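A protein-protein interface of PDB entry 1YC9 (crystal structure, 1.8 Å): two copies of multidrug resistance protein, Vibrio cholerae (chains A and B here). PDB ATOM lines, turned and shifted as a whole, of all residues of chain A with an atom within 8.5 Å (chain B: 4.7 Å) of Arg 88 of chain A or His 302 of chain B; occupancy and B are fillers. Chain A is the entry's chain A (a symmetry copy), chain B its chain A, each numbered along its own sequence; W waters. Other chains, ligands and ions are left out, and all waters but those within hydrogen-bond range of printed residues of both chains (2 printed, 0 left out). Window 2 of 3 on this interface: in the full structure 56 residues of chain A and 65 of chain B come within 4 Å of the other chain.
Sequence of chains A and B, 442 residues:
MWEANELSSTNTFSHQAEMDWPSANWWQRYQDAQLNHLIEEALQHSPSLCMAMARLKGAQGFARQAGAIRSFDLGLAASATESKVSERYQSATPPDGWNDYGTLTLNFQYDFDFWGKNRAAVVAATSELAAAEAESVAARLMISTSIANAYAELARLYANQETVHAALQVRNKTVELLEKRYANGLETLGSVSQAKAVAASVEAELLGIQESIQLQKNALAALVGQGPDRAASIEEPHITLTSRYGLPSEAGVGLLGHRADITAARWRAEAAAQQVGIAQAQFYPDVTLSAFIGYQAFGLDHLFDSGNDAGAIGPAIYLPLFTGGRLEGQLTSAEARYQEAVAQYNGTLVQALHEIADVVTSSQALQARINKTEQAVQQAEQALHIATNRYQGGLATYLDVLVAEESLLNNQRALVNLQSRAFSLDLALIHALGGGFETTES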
ATOM      1  N   LYS A  84       0.910  23.756 -26.829  1.00  0.00           N
ATOM      2  CA  LYS A  84       0.661  22.391 -26.471  1.00  0.00           C
ATOM      3  C   LYS A  84       0.738  22.351 -24.945  1.00  0.00           C
ATOM      4  O   LYS A  84       1.722  22.819 -24.401  1.00  0.00           O
ATOM      5  CB  LYS A  84       1.712  21.453 -26.976  1.00  0.00           C
ATOM      6  CG  LYS A  84       1.277  20.046 -26.790  1.00  0.00           C
ATOM      7  CD  LYS A  84       2.202  19.232 -26.070  1.00  0.00           C
ATOM      8  CE  LYS A  84       1.679  17.765 -25.960  1.00  0.00           C
ATOM      9  NZ  LYS A  84       1.714  17.381 -24.537  1.00  0.00           N
ATOM     10  N   VAL A  85      -0.323  21.890 -24.330  1.00  0.00           N
ATOM     11  CA  VAL A  85      -0.399  21.780 -22.847  1.00  0.00           C
ATOM     12  C   VAL A  85       0.088  20.390 -22.467  1.00  0.00           C
ATOM     13  O   VAL A  85      -0.191  19.382 -23.154  1.00  0.00           O
ATOM     14  CB  VAL A  85      -1.853  22.020 -22.407  1.00  0.00           C
ATOM     15  CG1 VAL A  85      -2.068  21.851 -20.902  1.00  0.00           C
ATOM     16  CG2 VAL A  85      -2.243  23.426 -22.811  1.00  0.00           C
ATOM     17  N   SER A  86       0.777  20.308 -21.324  1.00  0.00           N
ATOM     18  CA  SER A  86       1.074  19.023 -20.745  1.00  0.00           C
ATOM     19  C   SER A  86      -0.211  18.208 -20.418  1.00  0.00           C
ATOM     20  O   SER A  86      -1.182  18.743 -19.894  1.00  0.00           O
ATOM     21  CB  SER A  86       1.931  19.198 -19.467  1.00  0.00           C
ATOM     22  OG  SER A  86       2.118  17.904 -18.896  1.00  0.00           O
ATOM     23  N   GLU A  87      -0.175  16.906 -20.649  1.00  0.00           N
ATOM     24  CA  GLU A  87      -1.352  16.083 -20.469  1.00  0.00           C
ATOM     25  C   GLU A  87      -1.676  15.871 -18.985  1.00  0.00           C
ATOM     26  O   GLU A  87      -2.837  15.625 -18.679  1.00  0.00           O
ATOM     27  CB  GLU A  87      -1.237  14.708 -21.103  1.00  0.00           C
ATOM     28  CG  GLU A  87      -1.355  14.732 -22.630  1.00  0.00           C
ATOM     29  CD  GLU A  87      -1.300  13.317 -23.218  1.00  0.00           C
ATOM     30  OE1 GLU A  87      -0.791  13.178 -24.330  1.00  0.00           O
ATOM     31  OE2 GLU A  87      -1.736  12.343 -22.560  1.00  0.00           O
ATOM     32  N   ARG A  88      -0.669  15.949 -18.128  1.00  0.00           N
ATOM     33  CA  ARG A  88      -0.841  15.610 -16.690  1.00  0.00           C
ATOM     34  C   ARG A  88      -0.054  16.589 -15.865  1.00  0.00           C
ATOM     35  O   ARG A  88       1.029  16.278 -15.344  1.00  0.00           O
ATOM     36  CB  ARG A  88      -0.429  14.143 -16.437  1.00  0.00           C
ATOM     37  CG  ARG A  88      -1.072  13.473 -15.164  1.00  0.00           C
ATOM     38  CD  ARG A  88      -1.147  11.860 -15.174  1.00  0.00           C
ATOM     39  NE  ARG A  88      -1.266  11.324 -13.803  1.00  0.00           N
ATOM     40  CZ  ARG A  88      -0.266  11.329 -12.885  1.00  0.00           C
ATOM     41  NH1 ARG A  88      -0.490  10.870 -11.654  1.00  0.00           N
ATOM     42  NH2 ARG A  88       0.950  11.793 -13.177  1.00  0.00           N
ATOM     43  N   TYR A  89      -0.596  17.801 -15.754  1.00  0.00           N
ATOM     44  CA  TYR A  89       0.086  18.862 -15.064  1.00  0.00           C
ATOM     45  C   TYR A  89      -0.958  19.618 -14.253  1.00  0.00           C
ATOM     46  O   TYR A  89      -1.126  19.331 -13.069  1.00  0.00           O
ATOM     47  CB  TYR A  89       0.860  19.781 -16.039  1.00  0.00           C
ATOM     48  CG  TYR A  89       1.521  20.973 -15.428  1.00  0.00           C
ATOM     49  CD1 TYR A  89       2.277  20.857 -14.266  1.00  0.00           C
ATOM     50  CD2 TYR A  89       1.431  22.233 -15.984  1.00  0.00           C
ATOM     51  CE1 TYR A  89       2.992  21.924 -13.751  1.00  0.00           C
ATOM     52  CE2 TYR A  89       2.071  23.333 -15.416  1.00  0.00           C
ATOM     53  CZ  TYR A  89       2.856  23.190 -14.287  1.00  0.00           C
ATOM     54  OH  TYR A  89       3.524  24.254 -13.715  1.00  0.00           O
ATOM     55  N   GLN A  90      -1.683  20.526 -14.887  1.00  0.00           N
ATOM     56  CA  GLN A  90      -2.645  21.385 -14.184  1.00  0.00           C
ATOM     57  C   GLN A  90      -4.099  21.284 -14.667  1.00  0.00           C
ATOM     58  O   GLN A  90      -5.010  21.819 -14.006  1.00  0.00           O
ATOM     59  CB  GLN A  90      -2.138  22.836 -14.217  1.00  0.00           C
ATOM     60  CG  GLN A  90      -1.061  23.023 -13.134  1.00  0.00           C
ATOM     61  CD  GLN A  90      -0.449  24.402 -13.028  1.00  0.00           C
ATOM     62  OE1 GLN A  90       0.213  24.702 -12.018  1.00  0.00           O
ATOM     63  NE2 GLN A  90      -0.639  25.228 -14.028  1.00  0.00           N
ATOM     64  N   SER A  91      -4.345  20.607 -15.786  1.00  0.00           N
ATOM     65  CA  SER A  91      -5.712  20.421 -16.309  1.00  0.00           C
ATOM     66  C   SER A  91      -6.066  18.955 -16.274  1.00  0.00           C
ATOM     67  O   SER A  91      -5.276  18.122 -16.696  1.00  0.00           O
ATOM     68  CB  SER A  91      -5.806  20.982 -17.738  1.00  0.00           C
ATOM     69  OG  SER A  91      -7.123  20.843 -18.288  1.00  0.00           O
ATOM     70  N   ALA A  92      -7.250  18.595 -15.775  1.00  0.00           N
ATOM     71  CA  ALA A  92      -7.672  17.199 -15.916  1.00  0.00           C
ATOM     72  C   ALA A  92      -8.188  16.885 -17.328  1.00  0.00           C
ATOM     73  O   ALA A  92      -8.173  15.712 -17.744  1.00  0.00           O
ATOM     74  CB  ALA A  92      -8.728  16.819 -14.860  1.00  0.00           C
ATOM     75  N   THR A  93      -8.638  17.909 -18.059  1.00  0.00           N
ATOM     76  CA  THR A  93      -9.143  17.696 -19.413  1.00  0.00           C
ATOM     77  C   THR A  93      -8.481  18.608 -20.448  1.00  0.00           C
ATOM     78  O   THR A  93      -9.139  19.402 -21.088  1.00  0.00           O
ATOM     79  CB  THR A  93     -10.717  17.811 -19.426  1.00  0.00           C
ATOM     80  OG1 THR A  93     -11.101  19.157 -19.173  1.00  0.00           O
ATOM     81  CG2 THR A  93     -11.334  17.016 -18.278  1.00  0.00           C
ATOM     82  N   PRO A  94      -7.162  18.461 -20.621  1.00  0.00           N
ATOM     83  CA  PRO A  94      -6.379  19.308 -21.515  1.00  0.00           C
ATOM     84  C   PRO A  94      -6.684  19.025 -22.989  1.00  0.00           C
ATOM     85  O   PRO A  94      -7.008  17.934 -23.352  1.00  0.00           O
ATOM     86  CB  PRO A  94      -4.928  18.916 -21.176  1.00  0.00           C
ATOM     87  CG  PRO A  94      -5.030  17.525 -20.742  1.00  0.00           C
ATOM     88  CD  PRO A  94      -6.318  17.422 -20.007  1.00  0.00           C
ATOM     89  N   GLN B 296       6.354  19.668 -18.064  1.00  0.00           N
ATOM     90  CA  GLN B 296       5.557  20.081 -16.887  1.00  0.00           C
ATOM     91  C   GLN B 296       4.798  18.857 -16.448  1.00  0.00           C
ATOM     92  O   GLN B 296       4.136  18.167 -17.226  1.00  0.00           O
ATOM     93  CB  GLN B 296       4.625  21.238 -17.267  1.00  0.00           C
ATOM     94  CG  GLN B 296       5.319  22.498 -17.683  1.00  0.00           C
ATOM     95  CD  GLN B 296       4.375  23.521 -18.284  1.00  0.00           C
ATOM     96  OE1 GLN B 296       3.311  23.163 -18.770  1.00  0.00           O
ATOM     97  NE2 GLN B 296       4.739  24.776 -18.186  1.00  0.00           N
ATOM     98  N   ALA B 297       4.809  18.564 -15.118  1.00  0.00           N
ATOM     99  CA  ALA B 297       4.117  17.436 -14.614  1.00  0.00           C
ATOM    100  C   ALA B 297       3.641  17.574 -13.158  1.00  0.00           C
ATOM    101  O   ALA B 297       4.311  18.221 -12.384  1.00  0.00           O
ATOM    102  CB  ALA B 297       4.997  16.160 -14.756  1.00  0.00           C
ATOM    103  N   PHE B 298       2.476  17.008 -12.938  1.00  0.00           N
ATOM    104  CA  PHE B 298       1.960  16.633 -11.607  1.00  0.00           C
ATOM    105  C   PHE B 298       2.729  15.368 -11.294  1.00  0.00           C
ATOM    106  O   PHE B 298       2.550  14.352 -11.978  1.00  0.00           O
ATOM    107  CB  PHE B 298       0.475  16.374 -11.759  1.00  0.00           C
ATOM    108  CG  PHE B 298      -0.197  15.940 -10.498  1.00  0.00           C
ATOM    109  CD1 PHE B 298      -0.861  16.869  -9.702  1.00  0.00           C
ATOM    110  CD2 PHE B 298      -0.198  14.621 -10.128  1.00  0.00           C
ATOM    111  CE1 PHE B 298      -1.495  16.472  -8.560  1.00  0.00           C
ATOM    112  CE2 PHE B 298      -0.853  14.233  -8.924  1.00  0.00           C
ATOM    113  CZ  PHE B 298      -1.489  15.170  -8.194  1.00  0.00           C
ATOM    114  N   GLY B 299       3.614  15.434 -10.319  1.00  0.00           N
ATOM    115  CA  GLY B 299       4.451  14.335  -9.904  1.00  0.00           C
ATOM    116  C   GLY B 299       5.820  14.486 -10.518  1.00  0.00           C
ATOM    117  O   GLY B 299       5.976  14.283 -11.724  1.00  0.00           O
ATOM    118  N   LEU B 300       6.816  14.844  -9.731  1.00  0.00           N
ATOM    119  CA  LEU B 300       8.170  15.023 -10.238  1.00  0.00           C
ATOM    120  C   LEU B 300       8.729  13.793 -10.918  1.00  0.00           C
ATOM    121  O   LEU B 300       9.496  13.922 -11.894  1.00  0.00           O
ATOM    122  CB  LEU B 300       9.137  15.373  -9.114  1.00  0.00           C
ATOM    123  CG  LEU B 300       8.971  16.749  -8.530  1.00  0.00           C
ATOM    124  CD1 LEU B 300       9.991  16.795  -7.368  1.00  0.00           C
ATOM    125  CD2 LEU B 300       9.273  17.805  -9.581  1.00  0.00           C
ATOM    126  N   ASP B 301       8.311  12.618 -10.440  1.00  0.00           N
ATOM    127  CA  ASP B 301       8.746  11.345 -11.062  1.00  0.00           C
ATOM    128  C   ASP B 301       8.075  11.115 -12.418  1.00  0.00           C
ATOM    129  O   ASP B 301       8.378  10.162 -13.125  1.00  0.00           O
ATOM    130  CB  ASP B 301       8.520  10.144 -10.170  1.00  0.00           C
ATOM    131  CG  ASP B 301       7.146  10.063  -9.626  1.00  0.00           C
ATOM    132  OD1 ASP B 301       6.471  11.096  -9.420  1.00  0.00           O
ATOM    133  OD2 ASP B 301       6.631   8.974  -9.305  1.00  0.00           O
ATOM    134  N   HIS B 302       7.142  11.980 -12.778  1.00  0.00           N
ATOM    135  CA  HIS B 302       6.499  11.917 -14.084  1.00  0.00           C
ATOM    136  C   HIS B 302       6.898  13.022 -15.058  1.00  0.00           C
ATOM    137  O   HIS B 302       6.235  13.154 -16.132  1.00  0.00           O
ATOM    138  CB  HIS B 302       4.990  11.933 -13.872  1.00  0.00           C
ATOM    139  CG  HIS B 302       4.468  10.699 -13.208  1.00  0.00           C
ATOM    140  ND1 HIS B 302       4.379   9.482 -13.853  1.00  0.00           N
ATOM    141  CD2 HIS B 302       3.991  10.498 -11.949  1.00  0.00           C
ATOM    142  CE1 HIS B 302       3.887   8.582 -13.010  1.00  0.00           C
ATOM    143  NE2 HIS B 302       3.645   9.176 -11.848  1.00  0.00           N
ATOM    144  N   LEU B 303       7.927  13.782 -14.710  1.00  0.00           N
ATOM    145  CA  LEU B 303       8.304  15.002 -15.427  1.00  0.00           C
ATOM    146  C   LEU B 303       8.545  14.714 -16.917  1.00  0.00           C
ATOM    147  O   LEU B 303       8.108  15.457 -17.793  1.00  0.00           O
ATOM    148  CB  LEU B 303       9.538  15.619 -14.825  1.00  0.00           C
ATOM    149  CG  LEU B 303       9.971  16.945 -15.396  1.00  0.00           C
ATOM    150  CD1 LEU B 303       8.836  18.000 -15.262  1.00  0.00           C
ATOM    151  CD2 LEU B 303      11.253  17.388 -14.736  1.00  0.00           C
ATOM    152  N   PHE B 304       9.153  13.553 -17.163  1.00  0.00           N
ATOM    153  CA  PHE B 304       9.530  13.170 -18.507  1.00  0.00           C
ATOM    154  C   PHE B 304       8.626  12.197 -19.252  1.00  0.00           C
ATOM    155  O   PHE B 304       8.964  11.840 -20.407  1.00  0.00           O
ATOM    156  CB  PHE B 304      10.971  12.658 -18.489  1.00  0.00           C
ATOM    157  CG  PHE B 304      11.940  13.611 -17.911  1.00  0.00           C
ATOM    158  CD1 PHE B 304      12.663  13.267 -16.771  1.00  0.00           C
ATOM    159  CD2 PHE B 304      12.174  14.844 -18.473  1.00  0.00           C
ATOM    160  CE1 PHE B 304      13.584  14.158 -16.202  1.00  0.00           C
ATOM    161  CE2 PHE B 304      13.104  15.743 -17.910  1.00  0.00           C
ATOM    162  CZ  PHE B 304      13.826  15.397 -16.793  1.00  0.00           C
ATOM    163  N   ASP B 305       7.494  11.840 -18.670  1.00  0.00           N
ATOM    164  CA  ASP B 305       6.517  10.925 -19.220  1.00  0.00           C
ATOM    165  C   ASP B 305       6.042  11.427 -20.561  1.00  0.00           C
ATOM    166  O   ASP B 305       5.850  12.639 -20.777  1.00  0.00           O
ATOM    167  CB  ASP B 305       5.228  10.808 -18.390  1.00  0.00           C
ATOM    168  CG  ASP B 305       5.421  10.004 -17.087  1.00  0.00           C
ATOM    169  OD1 ASP B 305       6.560   9.678 -16.741  1.00  0.00           O
ATOM    170  OD2 ASP B 305       4.482   9.661 -16.395  1.00  0.00           O
ATOM    171  N   ASN B 308       3.707  14.795 -21.310  1.00  0.00           N
ATOM    172  CA  ASN B 308       4.000  15.874 -20.365  1.00  0.00           C
ATOM    173  C   ASN B 308       4.918  16.886 -20.898  1.00  0.00           C
ATOM    174  O   ASN B 308       5.375  17.771 -20.196  1.00  0.00           O
ATOM    175  CB  ASN B 308       4.495  15.316 -19.003  1.00  0.00           C
ATOM    176  CG  ASN B 308       3.400  14.556 -18.285  1.00  0.00           C
ATOM    177  OD1 ASN B 308       2.263  14.562 -18.716  1.00  0.00           O
ATOM    178  ND2 ASN B 308       3.749  13.919 -17.140  1.00  0.00           N
HETATM  179  O   HOH W   1       2.166  13.804 -14.652  1.00  0.00           O
HETATM  180  O   HOH W   2       0.945  22.822 -19.851  1.00  0.00           O
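OD1 of Asn 308 of chain B lies close to OG of Ser 86 of chain A (3.3 Å). The backbone NH of Phe 298 of chain B lies within hydrogen-bond range of the backbone carbonyl oxygen of Arg 88 of chain A (2.9 Å). The side-chain hydroxyl (OG) of Ser 86 of chain A lies within hydrogen-bond range of the backbone carbonyl oxygen (O) of Gln 296 of chain B (2.6 Å). N of Arg 88 of chain A sits at hydrogen-bond distance from OD1 of Asn 308 of chain B (3.3 Å).
N of Gln 296 of chain B lies within hydrogen-bond range of O of Asn 308 of chain B, 3.0 Å away. OG of Ser 86 of chain A sits close to N of Arg 88 of chain A (3.5 Å). ND2 of Asn 308 of chain B sits at hydrogen-bond distance from O of His 302 of chain B (2.8 Å). A ring nitrogen (ND1) of His 302 of chain B lies within hydrogen-bond range of the side-chain carboxylate (OD2) of Asp 305 of chain B.
N of Glu 87 of chain A touches OD1 of Asn 308 of chain B (3.9 Å). Arg 88 of chain A touches Ala 297 of chain B. CD2 of His 302 of chain B touches NH2 of Arg 88 of chain A, at 3.5 Å. Tyr 89 of chain A touches Gln 296 of chain B (CD2 to OE1, 3.5 Å). Tyr 89 of chain A touches Ala 297 of chain B. Phe 298 of chain B touches Tyr 89 of chain A.
Of the printed residues of chain B, Arg 88 of chain A touches Ala 297, Phe 298, His 302 and Asn 308. Of chain A, only Arg 88 (3.5 Å) comes within 4 Å of His 302 of chain B. Printed residues of chain B within 4 Å of Glu 87 of chain A: Asn 308. Of the printed residues of chain A, Asn 308 of chain B touches Ser 86, Glu 87 and Arg 88. Of the printed residues of chain A, Phe 298 of chain B touches Arg 88 (2.9 Å) and Tyr 89 (3.6 Å). Of the printed residues of chain B, Ser 86 of chain A touches Gln 296 (2.6 Å) and Asn 308 (3.1 Å). Printed residues of chain B within 4 Å of Tyr 89 of chain A: Gln 296 (3.5 Å), Ala 297 (3.5 Å) and Phe 298 (3.6 Å). Ser 91 of chain A touches none of the printed residues of chain B. The nearest residue of chain A that does not touch His 302 of chain B is Ser 86 of chain A (6.9 Å). The nearest printed residue of chain A that does not touch Ala 297 of chain B is Ser 86 of chain A (4.7 Å).
Hydrophobic or aromatic side chains of chain A that line the printed part of chain B: Tyr 89. Along chain A the printed residues that touch a printed residue of chain B span positions 86 to 89. Hydrophobic or aromatic side chains of chain B within 4 Å of the printed part of chain A: Phe 298 and His 302. Along chain B the printed residues that touch a printed residue of chain A span positions 296 to 308. Among the printed residues, 10 pairs touch across the chains.
No position is printed for both chains. Of the 10 pairs that touch across the chains among the printed residues, none has its exchanged pair printed and touching as well.
Water W2 lies within hydrogen-bond range of the side-chain amide oxygen (OE1) of Gln 296 of chain B (2.6 Å) and the backbone NH (N) of Ser 86 of chain A (2.9 Å). Water W1 lies within hydrogen-bond range of O of Phe 298 of chain B (2.8 Å), NH2 of Arg 88 of chain A (2.8 Å) and ND2 of Asn 308 of chain B (3.0 Å).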
